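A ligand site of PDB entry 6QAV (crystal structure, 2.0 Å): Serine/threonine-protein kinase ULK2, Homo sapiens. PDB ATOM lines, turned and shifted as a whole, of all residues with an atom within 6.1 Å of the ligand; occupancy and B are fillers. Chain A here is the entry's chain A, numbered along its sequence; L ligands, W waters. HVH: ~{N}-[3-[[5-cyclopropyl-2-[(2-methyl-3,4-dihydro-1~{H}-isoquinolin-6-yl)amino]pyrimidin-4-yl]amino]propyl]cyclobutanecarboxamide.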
ATOM      1  N   LEU A  18     -17.435   7.778  10.357  1.00  0.00           N
ATOM      2  CA  LEU A  18     -17.547   6.299  10.300  1.00  0.00           C
ATOM      3  C   LEU A  18     -17.048   5.709  11.627  1.00  0.00           C
ATOM      4  O   LEU A  18     -16.022   6.077  12.069  1.00  0.00           O
ATOM      5  CB  LEU A  18     -16.699   5.802   9.108  1.00  0.00           C
ATOM      6  CG  LEU A  18     -16.733   4.299   8.841  1.00  0.00           C
ATOM      7  CD1 LEU A  18     -18.084   3.900   8.278  1.00  0.00           C
ATOM      8  CD2 LEU A  18     -15.619   3.887   7.900  1.00  0.00           C
ATOM      9  N   VAL A  19     -17.820   4.811  12.244  1.00  0.00           N
ATOM     10  CA  VAL A  19     -17.348   4.189  13.496  1.00  0.00           C
ATOM     11  C   VAL A  19     -17.193   2.658  13.349  1.00  0.00           C
ATOM     12  O   VAL A  19     -16.586   2.029  14.215  1.00  0.00           O
ATOM     13  CB  VAL A  19     -18.247   4.551  14.688  1.00  0.00           C
ATOM     14  CG1 VAL A  19     -18.142   6.031  15.019  1.00  0.00           C
ATOM     15  CG2 VAL A  19     -19.686   4.139  14.471  1.00  0.00           C
ATOM     16  N   GLY A  20     -17.744   2.063  12.287  1.00  0.00           N
ATOM     17  CA  GLY A  20     -17.558   0.664  12.079  1.00  0.00           C
ATOM     18  C   GLY A  20     -17.939   0.244  10.686  1.00  0.00           C
ATOM     19  O   GLY A  20     -18.681   1.009   9.982  1.00  0.00           O
ATOM     20  N   HIS A  21     -17.407  -0.911  10.239  1.00  0.00           N
ATOM     21  CA  HIS A  21     -17.841  -1.475   8.996  1.00  0.00           C
ATOM     22  C   HIS A  21     -17.671  -2.977   9.018  1.00  0.00           C
ATOM     23  O   HIS A  21     -16.841  -3.469   9.682  1.00  0.00           O
ATOM     24  CB  HIS A  21     -17.116  -0.822   7.807  1.00  0.00           C
ATOM     25  CG  HIS A  21     -15.675  -1.171   7.741  1.00  0.00           C
ATOM     26  ND1 HIS A  21     -14.709  -0.496   8.482  1.00  0.00           N
ATOM     27  CD2 HIS A  21     -15.032  -2.166   7.072  1.00  0.00           C
ATOM     28  CE1 HIS A  21     -13.539  -1.072   8.268  1.00  0.00           C
ATOM     29  NE2 HIS A  21     -13.712  -2.081   7.388  1.00  0.00           N
ATOM     30  N   GLY A  22     -18.507  -3.660   8.269  1.00  0.00           N
ATOM     31  CA  GLY A  22     -18.351  -5.050   7.913  1.00  0.00           C
ATOM     32  C   GLY A  22     -18.533  -5.236   6.423  1.00  0.00           C
ATOM     33  O   GLY A  22     -18.557  -4.260   5.596  1.00  0.00           O
ATOM     34  N   ALA A  25     -22.156  -3.776   5.686  1.00  0.00           N
ATOM     35  CA  ALA A  25     -22.717  -2.723   6.519  1.00  0.00           C
ATOM     36  C   ALA A  25     -21.659  -1.660   6.866  1.00  0.00           C
ATOM     37  O   ALA A  25     -20.476  -1.994   7.050  1.00  0.00           O
ATOM     38  CB  ALA A  25     -23.326  -3.311   7.785  1.00  0.00           C
ATOM     39  N   VAL A  26     -22.123  -0.407   7.004  1.00  0.00           N
ATOM     40  CA  VAL A  26     -21.340   0.645   7.560  1.00  0.00           C
ATOM     41  C   VAL A  26     -22.145   1.350   8.655  1.00  0.00           C
ATOM     42  O   VAL A  26     -23.373   1.368   8.606  1.00  0.00           O
ATOM     43  CB  VAL A  26     -20.883   1.636   6.460  1.00  0.00           C
ATOM     44  CG1 VAL A  26     -19.868   1.009   5.538  1.00  0.00           C
ATOM     45  CG2 VAL A  26     -22.054   2.196   5.674  1.00  0.00           C
ATOM     46  N   VAL A  27     -21.434   1.818   9.672  1.00  0.00           N
ATOM     47  CA  VAL A  27     -22.048   2.451  10.792  1.00  0.00           C
ATOM     48  C   VAL A  27     -21.389   3.801  10.986  1.00  0.00           C
ATOM     49  O   VAL A  27     -20.171   3.867  11.044  1.00  0.00           O
ATOM     50  CB  VAL A  27     -21.949   1.616  12.092  1.00  0.00           C
ATOM     51  CG1 VAL A  27     -22.661   2.332  13.245  1.00  0.00           C
ATOM     52  CG2 VAL A  27     -22.480   0.194  11.930  1.00  0.00           C
ATOM     53  N   ALA A  41     -26.285   6.059  16.414  1.00  0.00           N
ATOM     54  CA  ALA A  41     -25.496   5.301  15.456  1.00  0.00           C
ATOM     55  C   ALA A  41     -26.399   4.922  14.294  1.00  0.00           C
ATOM     56  O   ALA A  41     -27.496   4.349  14.523  1.00  0.00           O
ATOM     57  CB  ALA A  41     -24.896   4.073  16.114  1.00  0.00           C
ATOM     58  N   LYS A  43     -26.664   2.726  10.893  1.00  0.00           N
ATOM     59  CA  LYS A  43     -26.123   1.589  10.196  1.00  0.00           C
ATOM     60  C   LYS A  43     -26.873   1.445   8.864  1.00  0.00           C
ATOM     61  O   LYS A  43     -28.108   1.426   8.860  1.00  0.00           O
ATOM     62  CB  LYS A  43     -26.359   0.329  11.025  1.00  0.00           C
ATOM     63  CG  LYS A  43     -25.832  -0.969  10.450  1.00  0.00           C
ATOM     64  CD  LYS A  43     -26.007  -2.114  11.424  1.00  0.00           C
ATOM     65  CE  LYS A  43     -25.343  -3.407  10.973  1.00  0.00           C
ATOM     66  NZ  LYS A  43     -25.497  -4.452  11.992  1.00  0.00           N
ATOM     67  N   GLU A  60     -31.732  -8.738  12.737  1.00  0.00           N
ATOM     68  CA  GLU A  60     -31.251  -7.726  13.697  1.00  0.00           C
ATOM     69  C   GLU A  60     -32.376  -6.770  14.126  1.00  0.00           C
ATOM     70  O   GLU A  60     -32.522  -6.472  15.274  1.00  0.00           O
ATOM     71  CB  GLU A  60     -30.045  -6.959  13.166  1.00  0.00           C
ATOM     72  CG  GLU A  60     -29.539  -5.924  14.156  1.00  0.00           C
ATOM     73  CD  GLU A  60     -28.175  -5.359  13.840  1.00  0.00           C
ATOM     74  OE1 GLU A  60     -27.924  -5.046  12.619  1.00  0.00           O
ATOM     75  OE2 GLU A  60     -27.375  -5.216  14.765  1.00  0.00           O
ATOM     76  N   VAL A  73     -27.780  -2.384  22.799  1.00  0.00           N
ATOM     77  CA  VAL A  73     -28.069  -1.160  22.031  1.00  0.00           C
ATOM     78  C   VAL A  73     -29.560  -1.108  21.672  1.00  0.00           C
ATOM     79  O   VAL A  73     -30.164  -2.101  21.178  1.00  0.00           O
ATOM     80  CB  VAL A  73     -27.190  -0.991  20.782  1.00  0.00           C
ATOM     81  CG1 VAL A  73     -25.755  -0.696  21.187  1.00  0.00           C
ATOM     82  CG2 VAL A  73     -27.289  -2.169  19.826  1.00  0.00           C
ATOM     83  N   ALA A  74     -30.157   0.051  21.955  1.00  0.00           N
ATOM     84  CA  ALA A  74     -31.540   0.363  21.577  1.00  0.00           C
ATOM     85  C   ALA A  74     -31.639   0.615  20.068  1.00  0.00           C
ATOM     86  O   ALA A  74     -30.695   1.099  19.435  1.00  0.00           O
ATOM     87  CB  ALA A  74     -32.022   1.575  22.349  1.00  0.00           C
ATOM     88  N   MET A  89     -29.801   3.582  15.838  1.00  0.00           N
ATOM     89  CA  MET A  89     -29.592   2.899  17.065  1.00  0.00           C
ATOM     90  C   MET A  89     -28.909   3.817  18.067  1.00  0.00           C
ATOM     91  O   MET A  89     -28.442   4.913  17.738  1.00  0.00           O
ATOM     92  CB  MET A  89     -28.747   1.653  16.802  1.00  0.00           C
ATOM     93  CG  MET A  89     -29.542   0.560  16.112  1.00  0.00           C
ATOM     94  SD  MET A  89     -28.584  -0.881  15.607  1.00  0.00           S
ATOM     95  CE  MET A  89     -27.512  -0.097  14.388  1.00  0.00           C
ATOM     96  N   GLU A  90     -28.843   3.314  19.306  1.00  0.00           N
ATOM     97  CA  GLU A  90     -28.125   3.947  20.409  1.00  0.00           C
ATOM     98  C   GLU A  90     -26.649   4.100  20.068  1.00  0.00           C
ATOM     99  O   GLU A  90     -26.011   3.145  19.614  1.00  0.00           O
ATOM    100  CB  GLU A  90     -28.267   3.064  21.632  1.00  0.00           C
ATOM    101  CG  GLU A  90     -27.765   3.673  22.921  1.00  0.00           C
ATOM    102  CD  GLU A  90     -28.140   2.804  24.107  1.00  0.00           C
ATOM    103  OE1 GLU A  90     -28.759   1.735  23.898  1.00  0.00           O
ATOM    104  OE2 GLU A  90     -27.760   3.183  25.234  1.00  0.00           O
ATOM    105  N   TYR A  91     -26.128   5.296  20.313  1.00  0.00           N
ATOM    106  CA  TYR A  91     -24.705   5.591  20.121  1.00  0.00           C
ATOM    107  C   TYR A  91     -23.958   5.376  21.451  1.00  0.00           C
ATOM    108  O   TYR A  91     -24.391   5.827  22.478  1.00  0.00           O
ATOM    109  CB  TYR A  91     -24.492   7.024  19.659  1.00  0.00           C
ATOM    110  CG  TYR A  91     -23.047   7.360  19.470  1.00  0.00           C
ATOM    111  CD1 TYR A  91     -22.291   6.761  18.476  1.00  0.00           C
ATOM    112  CD2 TYR A  91     -22.424   8.302  20.277  1.00  0.00           C
ATOM    113  CE1 TYR A  91     -20.951   7.081  18.285  1.00  0.00           C
ATOM    114  CE2 TYR A  91     -21.088   8.619  20.103  1.00  0.00           C
ATOM    115  CZ  TYR A  91     -20.353   8.002  19.099  1.00  0.00           C
ATOM    116  OH  TYR A  91     -19.029   8.261  18.909  1.00  0.00           O
ATOM    117  N   CYS A  92     -22.835   4.665  21.378  1.00  0.00           N
ATOM    118  CA  CYS A  92     -22.005   4.381  22.508  1.00  0.00           C
ATOM    119  C   CYS A  92     -20.768   5.267  22.397  1.00  0.00           C
ATOM    120  O   CYS A  92     -19.873   5.009  21.575  1.00  0.00           O
ATOM    121  CB  CYS A  92     -21.649   2.888  22.541  1.00  0.00           C
ATOM    122  SG  CYS A  92     -23.120   1.851  22.738  1.00  0.00           S
ATOM    123  N   ASN A  93     -20.703   6.285  23.254  1.00  0.00           N
ATOM    124  CA  ASN A  93     -19.745   7.392  23.070  1.00  0.00           C
ATOM    125  C   ASN A  93     -18.329   6.970  23.495  1.00  0.00           C
ATOM    126  O   ASN A  93     -17.403   7.742  23.303  1.00  0.00           O
ATOM    127  CB  ASN A  93     -20.200   8.659  23.806  1.00  0.00           C
ATOM    128  CG  ASN A  93     -20.351   8.472  25.302  1.00  0.00           C
ATOM    129  OD1 ASN A  93     -19.994   7.419  25.856  1.00  0.00           O
ATOM    130  ND2 ASN A  93     -20.936   9.462  25.943  1.00  0.00           N
ATOM    131  N   GLY A  94     -18.154   5.772  24.072  1.00  0.00           N
ATOM    132  CA  GLY A  94     -16.870   5.327  24.504  1.00  0.00           C
ATOM    133  C   GLY A  94     -16.146   4.447  23.484  1.00  0.00           C
ATOM    134  O   GLY A  94     -15.057   3.986  23.743  1.00  0.00           O
ATOM    135  N   GLY A  95     -16.783   4.105  22.367  1.00  0.00           N
ATOM    136  CA  GLY A  95     -16.123   3.156  21.425  1.00  0.00           C
ATOM    137  C   GLY A  95     -16.289   1.697  21.877  1.00  0.00           C
ATOM    138  O   GLY A  95     -17.249   1.364  22.647  1.00  0.00           O
ATOM    139  N   ASP A  96     -15.400   0.817  21.386  1.00  0.00           N
ATOM    140  CA  ASP A  96     -15.557  -0.595  21.642  1.00  0.00           C
ATOM    141  C   ASP A  96     -14.519  -1.058  22.663  1.00  0.00           C
ATOM    142  O   ASP A  96     -13.602  -0.311  23.051  1.00  0.00           O
ATOM    143  CB  ASP A  96     -15.516  -1.414  20.348  1.00  0.00           C
ATOM    144  CG  ASP A  96     -14.181  -1.328  19.623  1.00  0.00           C
ATOM    145  OD1 ASP A  96     -13.197  -0.921  20.233  1.00  0.00           O
ATOM    146  OD2 ASP A  96     -14.131  -1.672  18.445  1.00  0.00           O
ATOM    147  N   ASP A  99     -10.829  -0.848  21.601  1.00  0.00           N
ATOM    148  CA  ASP A  99     -10.218   0.482  21.765  1.00  0.00           C
ATOM    149  C   ASP A  99      -9.781   0.661  23.233  1.00  0.00           C
ATOM    150  O   ASP A  99      -8.709   1.195  23.521  1.00  0.00           O
ATOM    151  CB  ASP A  99     -11.177   1.626  21.437  1.00  0.00           C
ATOM    152  CG  ASP A  99     -11.743   1.616  20.012  1.00  0.00           C
ATOM    153  OD1 ASP A  99     -11.016   1.162  19.084  1.00  0.00           O
ATOM    154  OD2 ASP A  99     -12.908   2.112  19.850  1.00  0.00           O
ATOM    155  N   GLN A 139     -14.948  -6.002  19.434  1.00  0.00           N
ATOM    156  CA  GLN A 139     -15.348  -4.976  18.465  1.00  0.00           C
ATOM    157  C   GLN A 139     -16.855  -4.700  18.534  1.00  0.00           C
ATOM    158  O   GLN A 139     -17.289  -3.703  17.995  1.00  0.00           O
ATOM    159  CB  GLN A 139     -14.962  -5.414  17.042  1.00  0.00           C
ATOM    160  CG  GLN A 139     -13.448  -5.378  16.753  1.00  0.00           C
ATOM    161  CD  GLN A 139     -12.651  -6.495  17.403  1.00  0.00           C
ATOM    162  OE1 GLN A 139     -13.150  -7.597  17.728  1.00  0.00           O
ATOM    163  NE2 GLN A 139     -11.366  -6.223  17.597  1.00  0.00           N
ATOM    164  N   ASN A 140     -17.656  -5.573  19.185  1.00  0.00           N
ATOM    165  CA  ASN A 140     -19.098  -5.293  19.322  1.00  0.00           C
ATOM    166  C   ASN A 140     -19.572  -5.339  20.777  1.00  0.00           C
ATOM    167  O   ASN A 140     -20.781  -5.345  21.058  1.00  0.00           O
ATOM    168  CB  ASN A 140     -19.924  -6.171  18.381  1.00  0.00           C
ATOM    169  CG  ASN A 140     -19.649  -7.645  18.511  1.00  0.00           C
ATOM    170  OD1 ASN A 140     -19.376  -8.119  19.611  1.00  0.00           O
ATOM    171  ND2 ASN A 140     -19.770  -8.372  17.394  1.00  0.00           N
ATOM    172  N   LEU A 142     -19.508  -2.650  23.444  1.00  0.00           N
ATOM    173  CA  LEU A 142     -19.319  -1.228  23.358  1.00  0.00           C
ATOM    174  C   LEU A 142     -19.429  -0.600  24.751  1.00  0.00           C
ATOM    175  O   LEU A 142     -20.105  -1.121  25.670  1.00  0.00           O
ATOM    176  CB  LEU A 142     -20.372  -0.625  22.406  1.00  0.00           C
ATOM    177  CG  LEU A 142     -20.421  -1.266  21.015  1.00  0.00           C
ATOM    178  CD1 LEU A 142     -21.340  -0.461  20.038  1.00  0.00           C
ATOM    179  CD2 LEU A 142     -19.009  -1.401  20.411  1.00  0.00           C
ATOM    180  N   ILE A 160     -24.042  -4.460  24.238  1.00  0.00           N
ATOM    181  CA  ILE A 160     -23.802  -5.407  23.211  1.00  0.00           C
ATOM    182  C   ILE A 160     -24.456  -4.879  21.925  1.00  0.00           C
ATOM    183  O   ILE A 160     -25.606  -4.409  21.951  1.00  0.00           O
ATOM    184  CB  ILE A 160     -24.348  -6.785  23.599  1.00  0.00           C
ATOM    185  CG1 ILE A 160     -23.803  -7.250  24.935  1.00  0.00           C
ATOM    186  CG2 ILE A 160     -24.048  -7.790  22.508  1.00  0.00           C
ATOM    187  CD1 ILE A 160     -22.307  -7.165  25.025  1.00  0.00           C
ATOM    188  N   ALA A 161     -23.746  -5.046  20.814  1.00  0.00           N
ATOM    189  CA  ALA A 161     -24.173  -4.575  19.512  1.00  0.00           C
ATOM    190  C   ALA A 161     -23.934  -5.648  18.445  1.00  0.00           C
ATOM    191  O   ALA A 161     -23.287  -6.712  18.716  1.00  0.00           O
ATOM    192  CB  ALA A 161     -23.440  -3.310  19.170  1.00  0.00           C
ATOM    193  N   ASP A 162     -24.399  -5.300  17.222  1.00  0.00           N
ATOM    194  CA  ASP A 162     -24.218  -6.046  15.983  1.00  0.00           C
ATOM    195  C   ASP A 162     -24.811  -7.467  16.061  1.00  0.00           C
ATOM    196  O   ASP A 162     -24.089  -8.426  16.186  1.00  0.00           O
ATOM    197  CB  ASP A 162     -22.769  -6.123  15.536  1.00  0.00           C
ATOM    198  CG  ASP A 162     -22.683  -6.633  14.100  1.00  0.00           C
ATOM    199  OD1 ASP A 162     -23.784  -6.765  13.395  1.00  0.00           O
ATOM    200  OD2 ASP A 162     -21.591  -6.931  13.679  1.00  0.00           O
HETATM  201  N1  HVH L   1     -21.257   0.445  15.930  1.00  0.00           N
HETATM  202  C2  HVH L   1     -19.931  -2.621  12.002  1.00  0.00           C
HETATM  203  N3  HVH L   1     -19.854   3.705  18.772  1.00  0.00           N
HETATM  204  C4  HVH L   1     -21.827  -3.625  12.194  1.00  0.00           C
HETATM  205  N4  HVH L   1     -13.572   3.060  17.427  1.00  0.00           N
HETATM  206  C5  HVH L   1     -19.679  -2.088  16.515  1.00  0.00           C
HETATM  207  C6  HVH L   1     -19.086  -0.692  16.314  1.00  0.00           C
HETATM  208  O   HVH L   1     -21.832  -2.134  14.698  1.00  0.00           O
HETATM  209  C   HVH L   1     -20.789  -2.751  14.427  1.00  0.00           C
HETATM  210  C1  HVH L   1     -20.584  -3.430  13.117  1.00  0.00           C
HETATM  211  C3  HVH L   1     -20.937  -3.278  10.991  1.00  0.00           C
HETATM  212  N   HVH L   1     -19.750  -2.836  15.266  1.00  0.00           N
HETATM  213  C7  HVH L   1     -19.903   0.245  15.425  1.00  0.00           C
HETATM  214  C8  HVH L   1     -21.527   1.237  16.971  1.00  0.00           C
HETATM  215  C21 HVH L   1     -22.812   1.318  17.489  1.00  0.00           C
HETATM  216  C22 HVH L   1     -23.982   0.615  16.832  1.00  0.00           C
HETATM  217  C24 HVH L   1     -24.480  -0.708  17.312  1.00  0.00           C
HETATM  218  C23 HVH L   1     -25.313   0.493  17.508  1.00  0.00           C
HETATM  219  C20 HVH L   1     -22.997   2.237  18.495  1.00  0.00           C
HETATM  220  N5  HVH L   1     -22.032   3.033  18.967  1.00  0.00           N
HETATM  221  C9  HVH L   1     -20.844   2.857  18.409  1.00  0.00           C
HETATM  222  N2  HVH L   1     -20.543   2.002  17.443  1.00  0.00           N
HETATM  223  C10 HVH L   1     -18.483   3.780  18.507  1.00  0.00           C
HETATM  224  C19 HVH L   1     -17.844   4.976  18.779  1.00  0.00           C
HETATM  225  C18 HVH L   1     -16.511   5.135  18.435  1.00  0.00           C
HETATM  226  C13 HVH L   1     -15.777   4.088  17.903  1.00  0.00           C
HETATM  227  C14 HVH L   1     -14.353   4.312  17.458  1.00  0.00           C
HETATM  228  C15 HVH L   1     -12.226   3.304  16.831  1.00  0.00           C
HETATM  229  C16 HVH L   1     -14.293   2.029  16.678  1.00  0.00           C
HETATM  230  C17 HVH L   1     -15.568   1.628  17.396  1.00  0.00           C
HETATM  231  C12 HVH L   1     -16.383   2.838  17.751  1.00  0.00           C
HETATM  232  C11 HVH L   1     -17.752   2.695  18.033  1.00  0.00           C
HETATM  233  O   HOH W   1     -24.383  -3.098  14.355  1.00  0.00           O
HETATM  234  O   HOH W   2     -26.315  -3.252  16.307  1.00  0.00           O
HETATM  235  O   HOH W   3     -17.504  -4.585  14.300  1.00  0.00           O
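OD2 of Asp 99 is in salt-bridge range of N4 of the ligand, 2.7 Å away.
A nitrogen (N3) of the ligand lies within hydrogen-bond range of the backbone carbonyl oxygen (O) of Cys 92 (3.1 Å).
A nitrogen (N5) of the ligand lies within hydrogen-bond range of the backbone NH (N) of Cys 92.
The backbone NH of Val 73 lies within hydrogen-bond range of the backbone carbonyl oxygen of Ile 160 (3.1 Å).
The backbone NH of Val 27 is in hydrogen-bond range of the backbone carbonyl oxygen of Gly 20, 2.9 Å away.
The backbone NH (N) of Ala 161 sits at hydrogen-bond distance from the backbone carbonyl oxygen (O) of Asn 140 (3.0 Å).
The side-chain amino group of Lys 43 is in salt-bridge range of the side-chain carboxylate of Glu 60 (2.6 Å).
NZ of Lys 43 is in salt-bridge range of OD1 of Asp 162 (3.2 Å).
O of Ala 74 lies within hydrogen-bond range of N of Glu 90 (2.9 Å).
N of Val 19 lies within hydrogen-bond range of O of Val 27 (2.8 Å).
N of Asp 99 sits at hydrogen-bond distance from OD1 of Asp 96 (2.7 Å).
O of Val 19 touches C17 of the ligand, 3.4 Å away.
Gly 20 touches the ligand.
His 21 touches the ligand (N to C2, 3.5 Å).
Gly 22 touches the ligand.
CB of Ala 25 touches C3 of the ligand, at 3.998 Å.
CG1 of Val 27 touches N1 of the ligand, 3.6 Å away.
Ala 41 touches the ligand (CB to C20, 3.6 Å).
CE of Lys 43 touches C4 of the ligand, at 3.7 Å.
Val 73 touches the ligand.
CB of Met 89 touches C23 of the ligand, at 3.7 Å.
Glu 90 touches the ligand.
Tyr 91 touches the ligand (OH to C19, 3.5 Å).
CA of Gly 95 touches C18 of the ligand, 3.6 Å away.
Asp 96 touches the ligand.
Gln 139 touches the ligand (O to C5, 3.2 Å).
Leu 142 touches the ligand (CD1 to C21, 3.4 Å).
Ala 161 touches the ligand (CB to C24, 3.4 Å).
Asp 162 touches the ligand (OD2 to C4, 3.6 Å).
Hydrophobic or aromatic side chains that line the ligand: Val 19, Ala 25, Val 27, Ala 41, Val 73, Met 89, Tyr 91, Leu 142 and Ala 161.
Water W1 lies within hydrogen-bond range of an oxygen (O) of the ligand (2.7 Å) and the side-chain amino group (NZ) of Lys 43 (2.9 Å).
Water W2 lies within hydrogen-bond range of OE2 of Glu 60 (2.7 Å), N of Asp 162 (3.0 Å) and SD of Met 89 (3.4 Å).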
